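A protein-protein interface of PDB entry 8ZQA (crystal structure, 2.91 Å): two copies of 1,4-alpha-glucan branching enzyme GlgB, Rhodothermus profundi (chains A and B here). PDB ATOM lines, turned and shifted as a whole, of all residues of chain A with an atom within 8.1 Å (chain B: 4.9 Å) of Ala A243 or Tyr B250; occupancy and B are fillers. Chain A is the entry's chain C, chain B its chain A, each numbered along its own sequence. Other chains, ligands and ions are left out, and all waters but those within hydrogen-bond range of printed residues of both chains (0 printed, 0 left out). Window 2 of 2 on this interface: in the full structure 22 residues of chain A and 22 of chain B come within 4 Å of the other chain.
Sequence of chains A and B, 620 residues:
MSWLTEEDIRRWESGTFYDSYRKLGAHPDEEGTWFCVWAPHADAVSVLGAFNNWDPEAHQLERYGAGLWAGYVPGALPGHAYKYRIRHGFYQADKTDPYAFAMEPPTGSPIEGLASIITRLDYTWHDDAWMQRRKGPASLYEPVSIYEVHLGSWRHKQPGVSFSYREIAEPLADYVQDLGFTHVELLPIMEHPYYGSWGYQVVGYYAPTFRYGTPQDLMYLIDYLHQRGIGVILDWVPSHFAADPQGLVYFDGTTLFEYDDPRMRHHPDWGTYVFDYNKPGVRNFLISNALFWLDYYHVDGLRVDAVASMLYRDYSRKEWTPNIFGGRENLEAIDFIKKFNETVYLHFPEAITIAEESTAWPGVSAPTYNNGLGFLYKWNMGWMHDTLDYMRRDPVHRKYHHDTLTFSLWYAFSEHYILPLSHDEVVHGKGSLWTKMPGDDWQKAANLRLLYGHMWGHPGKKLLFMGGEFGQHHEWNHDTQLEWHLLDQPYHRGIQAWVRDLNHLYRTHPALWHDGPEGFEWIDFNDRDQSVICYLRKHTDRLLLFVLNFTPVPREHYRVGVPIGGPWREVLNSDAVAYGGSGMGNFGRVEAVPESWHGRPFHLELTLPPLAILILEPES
Pro A245 touches Tyr B250 (CB to CG, 3.7 Å).
O of Gly B253 touches CG of Pro A245 (2.9 Å).
Tyr B250 touches Tyr A273 (CE2 to OH, 3.97 Å).
Thr B272 touches Tyr A273.
Hydrophobic or aromatic side chains of chain B within 4 Å of the printed part of chain A: Tyr B250.
Hydrophobic or aromatic side chains of chain A that line the printed part of chain B: Pro A245 and Tyr A273.
Among the printed residues, no Asp or Glu carboxylate lies within 4 Å of a Lys or Arg side-chain nitrogen of the other chain.
OH of Tyr B250 lies within hydrogen-bond range of O of Ala A243, 2.5 Å away.
The side-chain carboxylate of Glu B258 lies within hydrogen-bond range of the backbone NH of Tyr B250 (2.6 Å).
Positions printed for both chains: 248, 249, 250 and 272.
Ala A243 touches just one residue of chain B: Tyr B250 (2.5 Å).
Of chain A, only Ala A243 (2.5 Å), Pro A245 (3.7 Å) and Tyr A273 (3.97 Å) come within 4 Å of Tyr B250.
Printed residues of chain B within 4 Å of Pro A245: Tyr B250 and Gly B253.
Printed residues of chain B within 4 Å of Tyr A273: Tyr B250 and Thr B272.
The nearest printed residue of chain B that does not touch Ala A243 is Thr B272 (5.3 Å).
The nearest residue of chain A that does not touch Tyr B250 is Asp A244 (4.8 Å).
The nearest printed residue of chain B that does not touch Tyr A273 is Val B249 (5.3 Å).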
ATOM      1  N   PRO A 193      -0.396   6.141 -28.144  1.00  0.00           N
ATOM      2  CA  PRO A 193      -1.379   5.058 -28.050  1.00  0.00           C
ATOM      3  C   PRO A 193      -2.555   5.303 -28.975  1.00  0.00           C
ATOM      4  O   PRO A 193      -2.991   4.420 -29.719  1.00  0.00           O
ATOM      5  CB  PRO A 193      -1.821   5.106 -26.578  1.00  0.00           C
ATOM      6  CG  PRO A 193      -1.075   6.280 -25.955  1.00  0.00           C
ATOM      7  CD  PRO A 193      -0.653   7.145 -27.104  1.00  0.00           C
ATOM      8  N   TYR A 200      -0.135  13.835 -30.954  1.00  0.00           N
ATOM      9  CA  TYR A 200       0.182  14.885 -29.995  1.00  0.00           C
ATOM     10  C   TYR A 200       0.100  14.420 -28.547  1.00  0.00           C
ATOM     11  O   TYR A 200       0.572  15.136 -27.657  1.00  0.00           O
ATOM     12  CB  TYR A 200      -0.724  16.094 -30.228  1.00  0.00           C
ATOM     13  CG  TYR A 200      -0.358  16.838 -31.492  1.00  0.00           C
ATOM     14  CD1 TYR A 200       0.632  17.813 -31.486  1.00  0.00           C
ATOM     15  CD2 TYR A 200      -0.978  16.543 -32.699  1.00  0.00           C
ATOM     16  CE1 TYR A 200       0.981  18.486 -32.643  1.00  0.00           C
ATOM     17  CE2 TYR A 200      -0.636  17.211 -33.860  1.00  0.00           C
ATOM     18  CZ  TYR A 200       0.345  18.181 -33.826  1.00  0.00           C
ATOM     19  OH  TYR A 200       0.687  18.848 -34.980  1.00  0.00           O
ATOM     20  N   GLN A 201      -0.476  13.249 -28.284  1.00  0.00           N
ATOM     21  CA  GLN A 201      -0.400  12.615 -26.969  1.00  0.00           C
ATOM     22  C   GLN A 201       0.654  11.517 -27.058  1.00  0.00           C
ATOM     23  O   GLN A 201       0.387  10.422 -27.555  1.00  0.00           O
ATOM     24  CB  GLN A 201      -1.761  12.076 -26.546  1.00  0.00           C
ATOM     25  CG  GLN A 201      -2.910  12.982 -26.945  1.00  0.00           C
ATOM     26  CD  GLN A 201      -2.901  14.287 -26.177  1.00  0.00           C
ATOM     27  OE1 GLN A 201      -2.703  14.302 -24.962  1.00  0.00           O
ATOM     28  NE2 GLN A 201      -3.094  15.393 -26.885  1.00  0.00           N
ATOM     29  N   VAL A 202       1.846  11.813 -26.542  1.00  0.00           N
ATOM     30  CA  VAL A 202       3.058  11.041 -26.808  1.00  0.00           C
ATOM     31  C   VAL A 202       3.391  10.189 -25.590  1.00  0.00           C
ATOM     32  O   VAL A 202       3.355  10.680 -24.455  1.00  0.00           O
ATOM     33  CB  VAL A 202       4.231  11.973 -27.156  1.00  0.00           C
ATOM     34  CG1 VAL A 202       5.434  11.170 -27.609  1.00  0.00           C
ATOM     35  CG2 VAL A 202       3.814  12.986 -28.215  1.00  0.00           C
ATOM     36  N   VAL A 203       3.732   8.920 -25.819  1.00  0.00           N
ATOM     37  CA  VAL A 203       4.214   8.032 -24.767  1.00  0.00           C
ATOM     38  C   VAL A 203       5.706   7.777 -24.919  1.00  0.00           C
ATOM     39  O   VAL A 203       6.466   7.867 -23.954  1.00  0.00           O
ATOM     40  CB  VAL A 203       3.451   6.689 -24.790  1.00  0.00           C
ATOM     41  CG1 VAL A 203       3.521   5.967 -23.439  1.00  0.00           C
ATOM     42  CG2 VAL A 203       2.099   6.839 -25.358  1.00  0.00           C
ATOM     43  N   HIS A 240       3.465  18.765 -23.257  1.00  0.00           N
ATOM     44  CA  HIS A 240       2.756  17.793 -22.437  1.00  0.00           C
ATOM     45  C   HIS A 240       3.039  16.389 -22.950  1.00  0.00           C
ATOM     46  O   HIS A 240       3.396  16.192 -24.115  1.00  0.00           O
ATOM     47  CB  HIS A 240       1.248  18.067 -22.434  1.00  0.00           C
ATOM     48  CG  HIS A 240       0.600  17.864 -23.766  1.00  0.00           C
ATOM     49  ND1 HIS A 240       0.622  18.824 -24.756  1.00  0.00           N
ATOM     50  CD2 HIS A 240      -0.087  16.815 -24.276  1.00  0.00           C
ATOM     51  CE1 HIS A 240      -0.022  18.373 -25.818  1.00  0.00           C
ATOM     52  NE2 HIS A 240      -0.465  17.157 -25.551  1.00  0.00           N
ATOM     53  N   PHE A 241       2.874  15.417 -22.059  1.00  0.00           N
ATOM     54  CA  PHE A 241       2.992  14.001 -22.373  1.00  0.00           C
ATOM     55  C   PHE A 241       1.628  13.334 -22.243  1.00  0.00           C
ATOM     56  O   PHE A 241       0.669  13.920 -21.734  1.00  0.00           O
ATOM     57  CB  PHE A 241       4.031  13.314 -21.474  1.00  0.00           C
ATOM     58  CG  PHE A 241       3.791  13.498 -20.001  1.00  0.00           C
ATOM     59  CD1 PHE A 241       3.016  12.594 -19.292  1.00  0.00           C
ATOM     60  CD2 PHE A 241       4.357  14.564 -19.321  1.00  0.00           C
ATOM     61  CE1 PHE A 241       2.803  12.756 -17.936  1.00  0.00           C
ATOM     62  CE2 PHE A 241       4.145  14.732 -17.967  1.00  0.00           C
ATOM     63  CZ  PHE A 241       3.367  13.827 -17.273  1.00  0.00           C
ATOM     64  N   ALA A 242       1.540  12.098 -22.731  1.00  0.00           N
ATOM     65  CA  ALA A 242       0.250  11.431 -22.800  1.00  0.00           C
ATOM     66  C   ALA A 242      -0.244  11.051 -21.408  1.00  0.00           C
ATOM     67  O   ALA A 242       0.537  10.781 -20.493  1.00  0.00           O
ATOM     68  CB  ALA A 242       0.338  10.180 -23.677  1.00  0.00           C
ATOM     69  N   ALA A 243      -1.569  11.025 -21.265  1.00  0.00           N
ATOM     70  CA  ALA A 243      -2.225  10.765 -19.990  1.00  0.00           C
ATOM     71  C   ALA A 243      -2.314   9.265 -19.745  1.00  0.00           C
ATOM     72  O   ALA A 243      -3.284   8.782 -19.145  1.00  0.00           O
ATOM     73  CB  ALA A 243      -3.618  11.400 -19.975  1.00  0.00           C
ATOM     74  N   ASP A 244      -1.282   8.521 -20.173  1.00  0.00           N
ATOM     75  CA  ASP A 244      -1.314   7.066 -20.263  1.00  0.00           C
ATOM     76  C   ASP A 244      -0.697   6.434 -19.021  1.00  0.00           C
ATOM     77  O   ASP A 244       0.451   6.741 -18.687  1.00  0.00           O
ATOM     78  CB  ASP A 244      -0.547   6.620 -21.500  1.00  0.00           C
ATOM     79  CG  ASP A 244      -1.039   5.312 -22.058  1.00  0.00           C
ATOM     80  OD1 ASP A 244      -0.617   4.257 -21.542  1.00  0.00           O
ATOM     81  OD2 ASP A 244      -1.839   5.336 -23.016  1.00  0.00           O
ATOM     82  N   PRO A 245      -1.387   5.471 -18.396  1.00  0.00           N
ATOM     83  CA  PRO A 245      -1.015   5.062 -17.025  1.00  0.00           C
ATOM     84  C   PRO A 245       0.346   4.402 -16.897  1.00  0.00           C
ATOM     85  O   PRO A 245       1.065   4.681 -15.930  1.00  0.00           O
ATOM     86  CB  PRO A 245      -2.148   4.099 -16.644  1.00  0.00           C
ATOM     87  CG  PRO A 245      -2.637   3.591 -17.949  1.00  0.00           C
ATOM     88  CD  PRO A 245      -2.556   4.734 -18.894  1.00  0.00           C
ATOM     89  N   GLN A 246       0.722   3.519 -17.824  1.00  0.00           N
ATOM     90  CA  GLN A 246       2.055   2.939 -17.757  1.00  0.00           C
ATOM     91  C   GLN A 246       3.124   3.888 -18.265  1.00  0.00           C
ATOM     92  O   GLN A 246       4.313   3.597 -18.104  1.00  0.00           O
ATOM     93  CB  GLN A 246       2.138   1.608 -18.516  1.00  0.00           C
ATOM     94  CG  GLN A 246       0.924   0.715 -18.383  1.00  0.00           C
ATOM     95  CD  GLN A 246      -0.137   1.005 -19.411  1.00  0.00           C
ATOM     96  OE1 GLN A 246      -0.367   2.155 -19.777  1.00  0.00           O
ATOM     97  NE2 GLN A 246      -0.798  -0.043 -19.883  1.00  0.00           N
ATOM     98  N   GLY A 247       2.739   5.022 -18.849  1.00  0.00           N
ATOM     99  CA  GLY A 247       3.715   5.908 -19.442  1.00  0.00           C
ATOM    100  C   GLY A 247       4.428   6.749 -18.405  1.00  0.00           C
ATOM    101  O   GLY A 247       4.775   6.255 -17.328  1.00  0.00           O
ATOM    102  N   LEU A 248       4.643   8.028 -18.710  1.00  0.00           N
ATOM    103  CA  LEU A 248       5.454   8.863 -17.833  1.00  0.00           C
ATOM    104  C   LEU A 248       4.692   9.375 -16.610  1.00  0.00           C
ATOM    105  O   LEU A 248       5.335   9.840 -15.662  1.00  0.00           O
ATOM    106  CB  LEU A 248       6.071  10.025 -18.626  1.00  0.00           C
ATOM    107  CG  LEU A 248       6.379   9.816 -20.117  1.00  0.00           C
ATOM    108  CD1 LEU A 248       6.936  11.095 -20.713  1.00  0.00           C
ATOM    109  CD2 LEU A 248       7.304   8.648 -20.391  1.00  0.00           C
ATOM    110  N   VAL A 249       3.352   9.335 -16.618  1.00  0.00           N
ATOM    111  CA  VAL A 249       2.569   9.756 -15.454  1.00  0.00           C
ATOM    112  C   VAL A 249       3.051   9.030 -14.209  1.00  0.00           C
ATOM    113  O   VAL A 249       3.097   7.797 -14.176  1.00  0.00           O
ATOM    114  CB  VAL A 249       1.061   9.514 -15.686  1.00  0.00           C
ATOM    115  CG1 VAL A 249       0.816   8.112 -16.160  1.00  0.00           C
ATOM    116  CG2 VAL A 249       0.275   9.758 -14.402  1.00  0.00           C
ATOM    117  N   TYR A 250       3.399   9.799 -13.182  1.00  0.00           N
ATOM    118  CA  TYR A 250       3.790   9.276 -11.875  1.00  0.00           C
ATOM    119  C   TYR A 250       4.744   8.090 -12.023  1.00  0.00           C
ATOM    120  O   TYR A 250       4.484   6.973 -11.571  1.00  0.00           O
ATOM    121  CB  TYR A 250       2.559   8.912 -11.035  1.00  0.00           C
ATOM    122  CG  TYR A 250       1.653  10.100 -10.790  1.00  0.00           C
ATOM    123  CD1 TYR A 250       2.188  11.338 -10.481  1.00  0.00           C
ATOM    124  CD2 TYR A 250       0.263   9.985 -10.861  1.00  0.00           C
ATOM    125  CE1 TYR A 250       1.389  12.425 -10.264  1.00  0.00           C
ATOM    126  CE2 TYR A 250      -0.555  11.092 -10.633  1.00  0.00           C
ATOM    127  CZ  TYR A 250       0.024  12.308 -10.334  1.00  0.00           C
ATOM    128  OH  TYR A 250      -0.746  13.424 -10.103  1.00  0.00           O
ATOM    129  N   TRP A 270      -3.602  21.539 -20.647  1.00  0.00           N
ATOM    130  CA  TRP A 270      -3.043  20.164 -20.510  1.00  0.00           C
ATOM    131  C   TRP A 270      -3.455  19.430 -19.228  1.00  0.00           C
ATOM    132  O   TRP A 270      -2.921  18.326 -18.988  1.00  0.00           O
ATOM    133  CB  TRP A 270      -1.516  20.213 -20.657  1.00  0.00           C
ATOM    134  CG  TRP A 270      -1.057  20.917 -21.906  1.00  0.00           C
ATOM    135  CD1 TRP A 270      -0.036  21.813 -22.002  1.00  0.00           C
ATOM    136  CD2 TRP A 270      -1.611  20.792 -23.234  1.00  0.00           C
ATOM    137  NE1 TRP A 270       0.091  22.250 -23.293  1.00  0.00           N
ATOM    138  CE2 TRP A 270      -0.862  21.646 -24.069  1.00  0.00           C
ATOM    139  CE3 TRP A 270      -2.653  20.049 -23.801  1.00  0.00           C
ATOM    140  CZ2 TRP A 270      -1.125  21.775 -25.429  1.00  0.00           C
ATOM    141  CZ3 TRP A 270      -2.918  20.183 -25.144  1.00  0.00           C
ATOM    142  CH2 TRP A 270      -2.163  21.035 -25.945  1.00  0.00           C
ATOM    143  N   THR A 272      -3.592  17.740 -15.820  1.00  0.00           N
ATOM    144  CA  THR A 272      -2.576  17.358 -14.816  1.00  0.00           C
ATOM    145  C   THR A 272      -1.214  17.141 -15.442  1.00  0.00           C
ATOM    146  O   THR A 272      -0.210  17.348 -14.730  1.00  0.00           O
ATOM    147  CB  THR A 272      -3.048  16.097 -14.095  1.00  0.00           C
ATOM    148  OG1 THR A 272      -4.463  16.219 -13.997  1.00  0.00           O
ATOM    149  CG2 THR A 272      -2.437  15.963 -12.712  1.00  0.00           C
ATOM    150  N   TYR A 273      -1.147  16.733 -16.711  1.00  0.00           N
ATOM    151  CA  TYR A 273       0.191  16.394 -17.263  1.00  0.00           C
ATOM    152  C   TYR A 273       0.837  17.553 -17.994  1.00  0.00           C
ATOM    153  O   TYR A 273       0.388  17.920 -19.093  1.00  0.00           O
ATOM    154  CB  TYR A 273      -0.072  15.193 -18.175  1.00  0.00           C
ATOM    155  CG  TYR A 273      -1.019  14.180 -17.546  1.00  0.00           C
ATOM    156  CD1 TYR A 273      -0.548  13.214 -16.668  1.00  0.00           C
ATOM    157  CD2 TYR A 273      -2.383  14.205 -17.809  1.00  0.00           C
ATOM    158  CE1 TYR A 273      -1.403  12.299 -16.079  1.00  0.00           C
ATOM    159  CE2 TYR A 273      -3.250  13.305 -17.213  1.00  0.00           C
ATOM    160  CZ  TYR A 273      -2.757  12.341 -16.355  1.00  0.00           C
ATOM    161  OH  TYR A 273      -3.599  11.438 -15.776  1.00  0.00           O
ATOM    162  N   LYS B  95      -2.461  -1.716  -6.105  1.00  0.00           N
ATOM    163  CA  LYS B  95      -3.490  -0.722  -5.828  1.00  0.00           C
ATOM    164  C   LYS B  95      -4.034  -0.888  -4.413  1.00  0.00           C
ATOM    165  O   LYS B  95      -3.982  -1.971  -3.826  1.00  0.00           O
ATOM    166  CB  LYS B  95      -4.661  -0.804  -6.822  1.00  0.00           C
ATOM    167  CG  LYS B  95      -4.365  -0.298  -8.221  1.00  0.00           C
ATOM    168  CD  LYS B  95      -3.521   0.956  -8.196  1.00  0.00           C
ATOM    169  CE  LYS B  95      -3.881   1.886  -9.339  1.00  0.00           C
ATOM    170  NZ  LYS B  95      -4.074   3.292  -8.885  1.00  0.00           N
ATOM    171  N   LEU B 248      -7.364   4.644  -6.711  1.00  0.00           N
ATOM    172  CA  LEU B 248      -8.495   5.103  -7.572  1.00  0.00           C
ATOM    173  C   LEU B 248      -8.085   5.339  -9.031  1.00  0.00           C
ATOM    174  O   LEU B 248      -8.543   4.568  -9.897  1.00  0.00           O
ATOM    175  CB  LEU B 248      -9.174   6.338  -6.978  1.00  0.00           C
ATOM    176  CG  LEU B 248     -10.433   6.089  -6.143  1.00  0.00           C
ATOM    177  CD1 LEU B 248     -11.650   6.749  -6.766  1.00  0.00           C
ATOM    178  CD2 LEU B 248     -10.682   4.611  -5.918  1.00  0.00           C
ATOM    179  N   VAL B 249      -7.303   6.381  -9.301  1.00  0.00           N
ATOM    180  CA  VAL B 249      -6.989   6.714 -10.717  1.00  0.00           C
ATOM    181  C   VAL B 249      -6.477   5.486 -11.474  1.00  0.00           C
ATOM    182  O   VAL B 249      -5.645   4.748 -10.910  1.00  0.00           O
ATOM    183  CB  VAL B 249      -5.872   7.764 -10.636  1.00  0.00           C
ATOM    184  CG1 VAL B 249      -5.497   8.308 -12.007  1.00  0.00           C
ATOM    185  CG2 VAL B 249      -6.194   8.878  -9.650  1.00  0.00           C
ATOM    186  N   TYR B 250      -6.957   5.300 -12.708  1.00  0.00           N
ATOM    187  CA  TYR B 250      -6.574   4.134 -13.555  1.00  0.00           C
ATOM    188  C   TYR B 250      -6.580   2.873 -12.715  1.00  0.00           C
ATOM    189  O   TYR B 250      -5.507   2.271 -12.518  1.00  0.00           O
ATOM    190  CB  TYR B 250      -5.237   4.417 -14.246  1.00  0.00           C
ATOM    191  CG  TYR B 250      -5.337   5.477 -15.332  1.00  0.00           C
ATOM    192  CD1 TYR B 250      -6.073   5.247 -16.485  1.00  0.00           C
ATOM    193  CD2 TYR B 250      -4.711   6.709 -15.199  1.00  0.00           C
ATOM    194  CE1 TYR B 250      -6.178   6.203 -17.479  1.00  0.00           C
ATOM    195  CE2 TYR B 250      -4.810   7.677 -16.185  1.00  0.00           C
ATOM    196  CZ  TYR B 250      -5.547   7.423 -17.328  1.00  0.00           C
ATOM    197  OH  TYR B 250      -5.655   8.363 -18.309  1.00  0.00           O
ATOM    198  N   PHE B 251      -7.761   2.446 -12.261  1.00  0.00           N
ATOM    199  CA  PHE B 251      -7.757   1.295 -11.365  1.00  0.00           C
ATOM    200  C   PHE B 251      -7.339   0.023 -12.098  1.00  0.00           C
ATOM    201  O   PHE B 251      -6.500  -0.741 -11.602  1.00  0.00           O
ATOM    202  CB  PHE B 251      -9.120   1.123 -10.696  1.00  0.00           C
ATOM    203  CG  PHE B 251      -9.048   0.374  -9.403  1.00  0.00           C
ATOM    204  CD1 PHE B 251      -8.297   0.870  -8.352  1.00  0.00           C
ATOM    205  CD2 PHE B 251      -9.702  -0.833  -9.243  1.00  0.00           C
ATOM    206  CE1 PHE B 251      -8.206   0.184  -7.164  1.00  0.00           C
ATOM    207  CE2 PHE B 251      -9.617  -1.525  -8.054  1.00  0.00           C
ATOM    208  CZ  PHE B 251      -8.862  -1.018  -7.016  1.00  0.00           C
ATOM    209  N   ASP B 252      -7.915  -0.235 -13.272  1.00  0.00           N
ATOM    210  CA  ASP B 252      -7.580  -1.441 -14.024  1.00  0.00           C
ATOM    211  C   ASP B 252      -6.328  -1.286 -14.856  1.00  0.00           C
ATOM    212  O   ASP B 252      -6.005  -2.190 -15.635  1.00  0.00           O
ATOM    213  CB  ASP B 252      -8.694  -1.784 -15.014  1.00  0.00           C
ATOM    214  CG  ASP B 252     -10.062  -1.651 -14.430  1.00  0.00           C
ATOM    215  OD1 ASP B 252     -10.487  -2.592 -13.752  1.00  0.00           O
ATOM    216  OD2 ASP B 252     -10.713  -0.608 -14.650  1.00  0.00           O
ATOM    217  N   GLY B 253      -5.604  -0.189 -14.704  1.00  0.00           N
ATOM    218  CA  GLY B 253      -4.630   0.164 -15.703  1.00  0.00           C
ATOM    219  C   GLY B 253      -5.236   1.000 -16.804  1.00  0.00           C
ATOM    220  O   GLY B 253      -4.520   1.413 -17.719  1.00  0.00           O
ATOM    221  N   THR B 254      -6.558   1.166 -16.791  1.00  0.00           N
ATOM    222  CA  THR B 254      -7.274   2.016 -17.726  1.00  0.00           C
ATOM    223  C   THR B 254      -8.266   2.851 -16.921  1.00  0.00           C
ATOM    224  O   THR B 254      -8.435   2.649 -15.714  1.00  0.00           O
ATOM    225  CB  THR B 254      -7.955   1.187 -18.823  1.00  0.00           C
ATOM    226  OG1 THR B 254      -8.851   2.013 -19.574  1.00  0.00           O
ATOM    227  CG2 THR B 254      -8.706   0.016 -18.221  1.00  0.00           C
ATOM    228  N   THR B 255      -8.979   3.745 -17.607  1.00  0.00           N
ATOM    229  CA  THR B 255      -9.969   4.589 -16.939  1.00  0.00           C
ATOM    230  C   THR B 255     -11.070   3.758 -16.292  1.00  0.00           C
ATOM    231  O   THR B 255     -11.656   2.879 -16.927  1.00  0.00           O
ATOM    232  CB  THR B 255     -10.591   5.581 -17.928  1.00  0.00           C
ATOM    233  OG1 THR B 255     -10.819   4.937 -19.188  1.00  0.00           O
ATOM    234  CG2 THR B 255      -9.699   6.794 -18.127  1.00  0.00           C
ATOM    235  N   GLU B 258     -12.628   7.456 -13.636  1.00  0.00           N
ATOM    236  CA  GLU B 258     -12.444   8.570 -14.548  1.00  0.00           C
ATOM    237  C   GLU B 258     -13.334   8.416 -15.776  1.00  0.00           C
ATOM    238  O   GLU B 258     -13.850   7.336 -16.074  1.00  0.00           O
ATOM    239  CB  GLU B 258     -10.988   8.644 -14.982  1.00  0.00           C
ATOM    240  CG  GLU B 258     -10.007   8.478 -13.839  1.00  0.00           C
ATOM    241  CD  GLU B 258      -9.200   7.194 -13.946  1.00  0.00           C
ATOM    242  OE1 GLU B 258      -9.797   6.100 -13.825  1.00  0.00           O
ATOM    243  OE2 GLU B 258      -7.972   7.274 -14.153  1.00  0.00           O
ATOM    244  N   THR B 272      -9.540  14.836 -15.109  1.00  0.00           N
ATOM    245  CA  THR B 272      -8.965  13.464 -15.065  1.00  0.00           C
ATOM    246  C   THR B 272      -9.100  12.926 -13.656  1.00  0.00           C
ATOM    247  O   THR B 272      -8.848  11.720 -13.455  1.00  0.00           O
ATOM    248  CB  THR B 272      -7.516  13.412 -15.563  1.00  0.00           C
ATOM    249  OG1 THR B 272      -7.432  14.237 -16.720  1.00  0.00           O
ATOM    250  CG2 THR B 272      -7.069  12.017 -15.963  1.00  0.00           C
